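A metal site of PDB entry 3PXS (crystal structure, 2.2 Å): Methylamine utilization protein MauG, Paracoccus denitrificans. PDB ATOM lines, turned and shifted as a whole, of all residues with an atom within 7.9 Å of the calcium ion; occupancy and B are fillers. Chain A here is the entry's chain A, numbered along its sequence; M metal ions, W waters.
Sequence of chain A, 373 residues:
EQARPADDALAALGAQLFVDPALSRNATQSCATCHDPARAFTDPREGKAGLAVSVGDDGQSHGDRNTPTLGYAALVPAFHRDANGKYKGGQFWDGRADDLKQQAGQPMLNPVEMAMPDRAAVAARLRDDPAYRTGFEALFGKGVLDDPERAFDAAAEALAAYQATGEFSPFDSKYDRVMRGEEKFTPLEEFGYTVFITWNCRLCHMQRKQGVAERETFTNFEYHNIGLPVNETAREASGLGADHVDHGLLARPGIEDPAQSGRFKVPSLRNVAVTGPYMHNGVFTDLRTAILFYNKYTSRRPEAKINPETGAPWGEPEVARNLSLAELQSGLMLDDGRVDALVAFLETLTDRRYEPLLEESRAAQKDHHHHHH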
ATOM      1  N   ARG A  39      13.198 -21.718  -1.350  1.00  0.00           N
ATOM      2  CA  ARG A  39      13.975 -21.626  -0.111  1.00  0.00           C
ATOM      3  C   ARG A  39      15.480 -21.418  -0.365  1.00  0.00           C
ATOM      4  O   ARG A  39      16.327 -22.129   0.182  1.00  0.00           O
ATOM      5  CB  ARG A  39      13.768 -22.864   0.773  1.00  0.00           C
ATOM      6  CG  ARG A  39      13.552 -22.530   2.244  1.00  0.00           C
ATOM      7  CD  ARG A  39      13.486 -23.755   3.133  1.00  0.00           C
ATOM      8  NE  ARG A  39      14.843 -24.152   3.514  1.00  0.00           N
ATOM      9  CZ  ARG A  39      15.325 -24.157   4.756  1.00  0.00           C
ATOM     10  NH1 ARG A  39      14.576 -23.839   5.802  1.00  0.00           N
ATOM     11  NH2 ARG A  39      16.588 -24.523   4.925  1.00  0.00           N
ATOM     12  N   THR A  42      17.593 -24.541  -1.153  1.00  0.00           N
ATOM     13  CA  THR A  42      17.835 -25.536  -0.105  1.00  0.00           C
ATOM     14  C   THR A  42      16.604 -26.425   0.090  1.00  0.00           C
ATOM     15  O   THR A  42      15.618 -26.300  -0.641  1.00  0.00           O
ATOM     16  CB  THR A  42      18.241 -24.903   1.244  1.00  0.00           C
ATOM     17  OG1 THR A  42      17.208 -24.008   1.672  1.00  0.00           O
ATOM     18  CG2 THR A  42      19.571 -24.171   1.136  1.00  0.00           C
ATOM     19  N   ASP A  43      16.663 -27.329   1.072  1.00  0.00           N
ATOM     20  CA  ASP A  43      15.636 -28.356   1.247  1.00  0.00           C
ATOM     21  C   ASP A  43      14.687 -28.067   2.436  1.00  0.00           C
ATOM     22  O   ASP A  43      15.105 -28.116   3.599  1.00  0.00           O
ATOM     23  CB  ASP A  43      16.306 -29.716   1.427  1.00  0.00           C
ATOM     24  CG  ASP A  43      15.347 -30.885   1.253  1.00  0.00           C
ATOM     25  OD1 ASP A  43      15.848 -32.019   1.197  1.00  0.00           O
ATOM     26  OD2 ASP A  43      14.114 -30.685   1.154  1.00  0.00           O
ATOM     27  N   LEU A  51      15.494 -30.879   9.338  1.00  0.00           N
ATOM     28  CA  LEU A  51      15.979 -30.310   8.084  1.00  0.00           C
ATOM     29  C   LEU A  51      17.498 -30.460   7.908  1.00  0.00           C
ATOM     30  O   LEU A  51      18.074 -29.957   6.940  1.00  0.00           O
ATOM     31  CB  LEU A  51      15.570 -28.839   7.985  1.00  0.00           C
ATOM     32  CG  LEU A  51      14.212 -28.444   7.391  1.00  0.00           C
ATOM     33  CD1 LEU A  51      13.021 -29.120   8.077  1.00  0.00           C
ATOM     34  CD2 LEU A  51      14.047 -26.930   7.446  1.00  0.00           C
ATOM     35  N   ALA A  52      18.127 -31.158   8.856  1.00  0.00           N
ATOM     36  CA  ALA A  52      19.586 -31.340   8.864  1.00  0.00           C
ATOM     37  C   ALA A  52      20.125 -32.027   7.609  1.00  0.00           C
ATOM     38  O   ALA A  52      21.152 -31.632   7.080  1.00  0.00           O
ATOM     39  CB  ALA A  52      20.028 -32.091  10.110  1.00  0.00           C
ATOM     40  N   ASN A  66      24.273 -31.520   5.415  1.00  0.00           N
ATOM     41  CA  ASN A  66      23.228 -30.561   5.080  1.00  0.00           C
ATOM     42  C   ASN A  66      23.320 -30.123   3.619  1.00  0.00           C
ATOM     43  O   ASN A  66      24.418 -29.928   3.078  1.00  0.00           O
ATOM     44  CB  ASN A  66      23.301 -29.336   6.007  1.00  0.00           C
ATOM     45  CG  ASN A  66      22.141 -28.389   5.829  1.00  0.00           C
ATOM     46  OD1 ASN A  66      22.325 -27.226   5.473  1.00  0.00           O
ATOM     47  ND2 ASN A  66      20.916 -28.887   6.056  1.00  0.00           N
ATOM     48  N   THR A  67      22.150 -29.990   2.986  1.00  0.00           N
ATOM     49  CA  THR A  67      22.059 -29.542   1.607  1.00  0.00           C
ATOM     50  C   THR A  67      22.300 -28.037   1.528  1.00  0.00           C
ATOM     51  O   THR A  67      21.512 -27.266   2.048  1.00  0.00           O
ATOM     52  CB  THR A  67      20.683 -29.883   1.007  1.00  0.00           C
ATOM     53  OG1 THR A  67      20.492 -31.311   1.035  1.00  0.00           O
ATOM     54  CG2 THR A  67      20.550 -29.386  -0.410  1.00  0.00           C
ATOM     55  N   PRO A  68      23.405 -27.619   0.873  1.00  0.00           N
ATOM     56  CA  PRO A  68      23.740 -26.199   0.798  1.00  0.00           C
ATOM     57  C   PRO A  68      23.007 -25.465  -0.326  1.00  0.00           C
ATOM     58  O   PRO A  68      22.497 -26.105  -1.243  1.00  0.00           O
ATOM     59  CB  PRO A  68      25.247 -26.213   0.504  1.00  0.00           C
ATOM     60  CG  PRO A  68      25.482 -27.502  -0.214  1.00  0.00           C
ATOM     61  CD  PRO A  68      24.344 -28.448   0.104  1.00  0.00           C
ATOM     62  N   THR A  69      22.960 -24.145  -0.243  1.00  0.00           N
ATOM     63  CA  THR A  69      22.398 -23.311  -1.310  1.00  0.00           C
ATOM     64  C   THR A  69      23.211 -23.394  -2.602  1.00  0.00           C
ATOM     65  O   THR A  69      24.410 -23.680  -2.578  1.00  0.00           O
ATOM     66  CB  THR A  69      22.309 -21.823  -0.871  1.00  0.00           C
ATOM     67  OG1 THR A  69      21.675 -21.060  -1.899  1.00  0.00           O
ATOM     68  CG2 THR A  69      23.703 -21.239  -0.576  1.00  0.00           C
ATOM     69  N   TRP A  93      30.761 -29.720   0.492  1.00  0.00           N
ATOM     70  CA  TRP A  93      31.275 -29.271   1.787  1.00  0.00           C
ATOM     71  C   TRP A  93      32.744 -29.648   1.953  1.00  0.00           C
ATOM     72  O   TRP A  93      33.463 -28.996   2.713  1.00  0.00           O
ATOM     73  CB  TRP A  93      30.461 -29.823   2.955  1.00  0.00           C
ATOM     74  CG  TRP A  93      29.116 -29.186   3.182  1.00  0.00           C
ATOM     75  CD1 TRP A  93      27.908 -29.671   2.784  1.00  0.00           C
ATOM     76  CD2 TRP A  93      28.841 -27.956   3.890  1.00  0.00           C
ATOM     77  NE1 TRP A  93      26.900 -28.832   3.183  1.00  0.00           N
ATOM     78  CE2 TRP A  93      27.440 -27.777   3.872  1.00  0.00           C
ATOM     79  CE3 TRP A  93      29.642 -27.015   4.537  1.00  0.00           C
ATOM     80  CZ2 TRP A  93      26.808 -26.663   4.462  1.00  0.00           C
ATOM     81  CZ3 TRP A  93      29.009 -25.904   5.144  1.00  0.00           C
ATOM     82  CH2 TRP A  93      27.611 -25.751   5.090  1.00  0.00           C
ATOM     83  N   ASN A 271      22.209 -15.224   1.897  1.00  0.00           N
ATOM     84  CA  ASN A 271      20.949 -15.919   2.225  1.00  0.00           C
ATOM     85  C   ASN A 271      20.997 -16.783   3.488  1.00  0.00           C
ATOM     86  O   ASN A 271      20.123 -17.616   3.711  1.00  0.00           O
ATOM     87  CB  ASN A 271      20.440 -16.754   1.043  1.00  0.00           C
ATOM     88  CG  ASN A 271      20.128 -15.916  -0.175  1.00  0.00           C
ATOM     89  OD1 ASN A 271      19.506 -14.847  -0.064  1.00  0.00           O
ATOM     90  ND2 ASN A 271      20.550 -16.387  -1.352  1.00  0.00           N
ATOM     91  N   VAL A 272      22.015 -16.574   4.323  1.00  0.00           N
ATOM     92  CA  VAL A 272      22.194 -17.391   5.515  1.00  0.00           C
ATOM     93  C   VAL A 272      20.965 -17.344   6.437  1.00  0.00           C
ATOM     94  O   VAL A 272      20.637 -18.342   7.090  1.00  0.00           O
ATOM     95  CB  VAL A 272      23.525 -17.059   6.276  1.00  0.00           C
ATOM     96  CG1 VAL A 272      23.475 -15.683   6.941  1.00  0.00           C
ATOM     97  CG2 VAL A 272      23.872 -18.157   7.282  1.00  0.00           C
ATOM     98  N   VAL A 274      17.915 -17.479   5.733  1.00  0.00           N
ATOM     99  CA  VAL A 274      16.802 -18.298   5.257  1.00  0.00           C
ATOM    100  C   VAL A 274      17.176 -19.740   4.874  1.00  0.00           C
ATOM    101  O   VAL A 274      16.348 -20.460   4.318  1.00  0.00           O
ATOM    102  CB  VAL A 274      16.028 -17.576   4.105  1.00  0.00           C
ATOM    103  CG1 VAL A 274      15.311 -16.362   4.648  1.00  0.00           C
ATOM    104  CG2 VAL A 274      16.966 -17.173   2.968  1.00  0.00           C
ATOM    105  N   THR A 275      18.403 -20.151   5.197  1.00  0.00           N
ATOM    106  CA  THR A 275      18.902 -21.476   4.806  1.00  0.00           C
ATOM    107  C   THR A 275      19.318 -22.375   5.981  1.00  0.00           C
ATOM    108  O   THR A 275      20.238 -23.194   5.843  1.00  0.00           O
ATOM    109  CB  THR A 275      20.106 -21.372   3.858  1.00  0.00           C
ATOM    110  OG1 THR A 275      21.183 -20.704   4.546  1.00  0.00           O
ATOM    111  CG2 THR A 275      19.758 -20.614   2.578  1.00  0.00           C
ATOM    112  N   GLY A 276      18.646 -22.222   7.124  1.00  0.00           N
ATOM    113  CA  GLY A 276      18.857 -23.102   8.268  1.00  0.00           C
ATOM    114  C   GLY A 276      18.323 -24.500   8.005  1.00  0.00           C
ATOM    115  O   GLY A 276      17.469 -24.671   7.129  1.00  0.00           O
ATOM    116  N   PRO A 277      18.782 -25.504   8.766  1.00  0.00           N
ATOM    117  CA  PRO A 277      19.747 -25.448   9.858  1.00  0.00           C
ATOM    118  C   PRO A 277      21.190 -25.277   9.361  1.00  0.00           C
ATOM    119  O   PRO A 277      21.437 -25.308   8.151  1.00  0.00           O
ATOM    120  CB  PRO A 277      19.577 -26.811  10.543  1.00  0.00           C
ATOM    121  CG  PRO A 277      19.149 -27.710   9.470  1.00  0.00           C
ATOM    122  CD  PRO A 277      18.331 -26.885   8.517  1.00  0.00           C
ATOM    123  N   TYR A 278      22.126 -25.115  10.292  1.00  0.00           N
ATOM    124  CA  TYR A 278      23.450 -24.608   9.954  1.00  0.00           C
ATOM    125  C   TYR A 278      24.599 -25.590  10.100  1.00  0.00           C
ATOM    126  O   TYR A 278      24.514 -26.566  10.831  1.00  0.00           O
ATOM    127  CB  TYR A 278      23.694 -23.299  10.714  1.00  0.00           C
ATOM    128  CG  TYR A 278      22.642 -22.288  10.350  1.00  0.00           C
ATOM    129  CD1 TYR A 278      21.581 -22.017  11.208  1.00  0.00           C
ATOM    130  CD2 TYR A 278      22.665 -21.663   9.106  1.00  0.00           C
ATOM    131  CE1 TYR A 278      20.589 -21.121  10.850  1.00  0.00           C
ATOM    132  CE2 TYR A 278      21.688 -20.768   8.749  1.00  0.00           C
ATOM    133  CZ  TYR A 278      20.653 -20.491   9.622  1.00  0.00           C
ATOM    134  OH  TYR A 278      19.692 -19.596   9.235  1.00  0.00           O
ATOM    135  N   MET A 279      25.670 -25.290   9.367  1.00  0.00           N
ATOM    136  CA  MET A 279      26.916 -26.073   9.339  1.00  0.00           C
ATOM    137  C   MET A 279      26.784 -27.311   8.458  1.00  0.00           C
ATOM    138  O   MET A 279      25.689 -27.644   8.007  1.00  0.00           O
ATOM    139  CB  MET A 279      27.392 -26.449  10.756  1.00  0.00           C
ATOM    140  CG  MET A 279      27.521 -25.263  11.719  1.00  0.00           C
ATOM    141  SD  MET A 279      28.691 -23.996  11.180  1.00  0.00           S
ATOM    142  CE  MET A 279      28.404 -22.732  12.416  1.00  0.00           C
ATOM    143  N   HIS A 280      27.912 -27.976   8.219  1.00  0.00           N
ATOM    144  CA  HIS A 280      27.978 -29.090   7.272  1.00  0.00           C
ATOM    145  C   HIS A 280      27.015 -30.224   7.603  1.00  0.00           C
ATOM    146  O   HIS A 280      26.641 -30.997   6.728  1.00  0.00           O
ATOM    147  CB  HIS A 280      29.400 -29.625   7.132  1.00  0.00           C
ATOM    148  CG  HIS A 280      29.906 -30.330   8.356  1.00  0.00           C
ATOM    149  ND1 HIS A 280      30.834 -29.757   9.210  1.00  0.00           N
ATOM    150  CD2 HIS A 280      29.644 -31.554   8.854  1.00  0.00           C
ATOM    151  CE1 HIS A 280      31.097 -30.605  10.191  1.00  0.00           C
ATOM    152  NE2 HIS A 280      30.386 -31.705   9.999  1.00  0.00           N
ATOM    153  N   ASN A 281      26.605 -30.320   8.876  1.00  0.00           N
ATOM    154  CA  ASN A 281      25.712 -31.388   9.316  1.00  0.00           C
ATOM    155  C   ASN A 281      24.383 -30.886   9.899  1.00  0.00           C
ATOM    156  O   ASN A 281      23.695 -31.619  10.623  1.00  0.00           O
ATOM    157  CB  ASN A 281      26.421 -32.295  10.333  1.00  0.00           C
ATOM    158  CG  ASN A 281      26.881 -31.542  11.552  1.00  0.00           C
ATOM    159  OD1 ASN A 281      26.417 -30.445  11.833  1.00  0.00           O
ATOM    160  ND2 ASN A 281      27.788 -32.143  12.312  1.00  0.00           N
ATOM    161  N   GLY A 282      24.043 -29.629   9.594  1.00  0.00           N
ATOM    162  CA  GLY A 282      22.791 -29.009  10.042  1.00  0.00           C
ATOM    163  C   GLY A 282      22.481 -29.105  11.522  1.00  0.00           C
ATOM    164  O   GLY A 282      21.322 -29.099  11.922  1.00  0.00           O
ATOM    165  N   PHE A 284      22.768 -27.000  14.035  1.00  0.00           N
ATOM    166  CA  PHE A 284      22.090 -25.852  14.654  1.00  0.00           C
ATOM    167  C   PHE A 284      20.908 -25.380  13.819  1.00  0.00           C
ATOM    168  O   PHE A 284      21.075 -25.003  12.657  1.00  0.00           O
ATOM    169  CB  PHE A 284      23.060 -24.693  14.879  1.00  0.00           C
ATOM    170  CG  PHE A 284      24.358 -25.102  15.521  1.00  0.00           C
ATOM    171  CD1 PHE A 284      24.378 -25.930  16.637  1.00  0.00           C
ATOM    172  CD2 PHE A 284      25.566 -24.636  15.007  1.00  0.00           C
ATOM    173  CE1 PHE A 284      25.566 -26.298  17.223  1.00  0.00           C
ATOM    174  CE2 PHE A 284      26.767 -24.995  15.590  1.00  0.00           C
ATOM    175  CZ  PHE A 284      26.774 -25.832  16.709  1.00  0.00           C
HETATM  176 CA    CA M   1      21.867 -25.000   5.765  1.00  0.00          CA
HETATM  177  O   HOH W   1      19.654 -26.126   5.348  1.00  0.00           O
HETATM  178  O   HOH W   2      22.698 -22.690   5.584  1.00  0.00           O
HETATM  179  O   HOH W   3      21.972 -24.985   3.407  1.00  0.00           O
HETATM  180  O   HOH W   4      24.198 -25.222   6.347  1.00  0.00           O
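The indole nitrogen of Trp 93 is in hydrogen-bond range of the backbone carbonyl oxygen of Asn 66 (2.7 Å).
The side-chain amide nitrogen of Asn 66 sits at hydrogen-bond distance from the backbone carbonyl oxygen of Leu 51, at 3.2 Å.
ND2 of Asn 66 is in hydrogen-bond range of O of Ala 52, 2.9 Å away.
N of Asn 66 lies within hydrogen-bond range of O of His 280.
The side-chain hydroxyl of Thr 275 sits close to the backbone carbonyl oxygen of Asn 271, 3.4 Å away.
Of the 22 residues printed, 3 come within 4 Å of the calcium ion.
The calcium ion is bound by the side-chain amide oxygen of Asn 66 (2.3 Å), water W3 (2.4 Å), water W4 (2.4 Å), the backbone carbonyl oxygen of Thr 275 (2.4 Å), the backbone carbonyl oxygen of Pro 277 (2.4 Å), water W2 (2.5 Å) and water W1 (2.5 Å).
Water W1 lies within hydrogen-bond range of ND2 of Asn 66, O of Gly 276 and NH2 of Arg 39.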
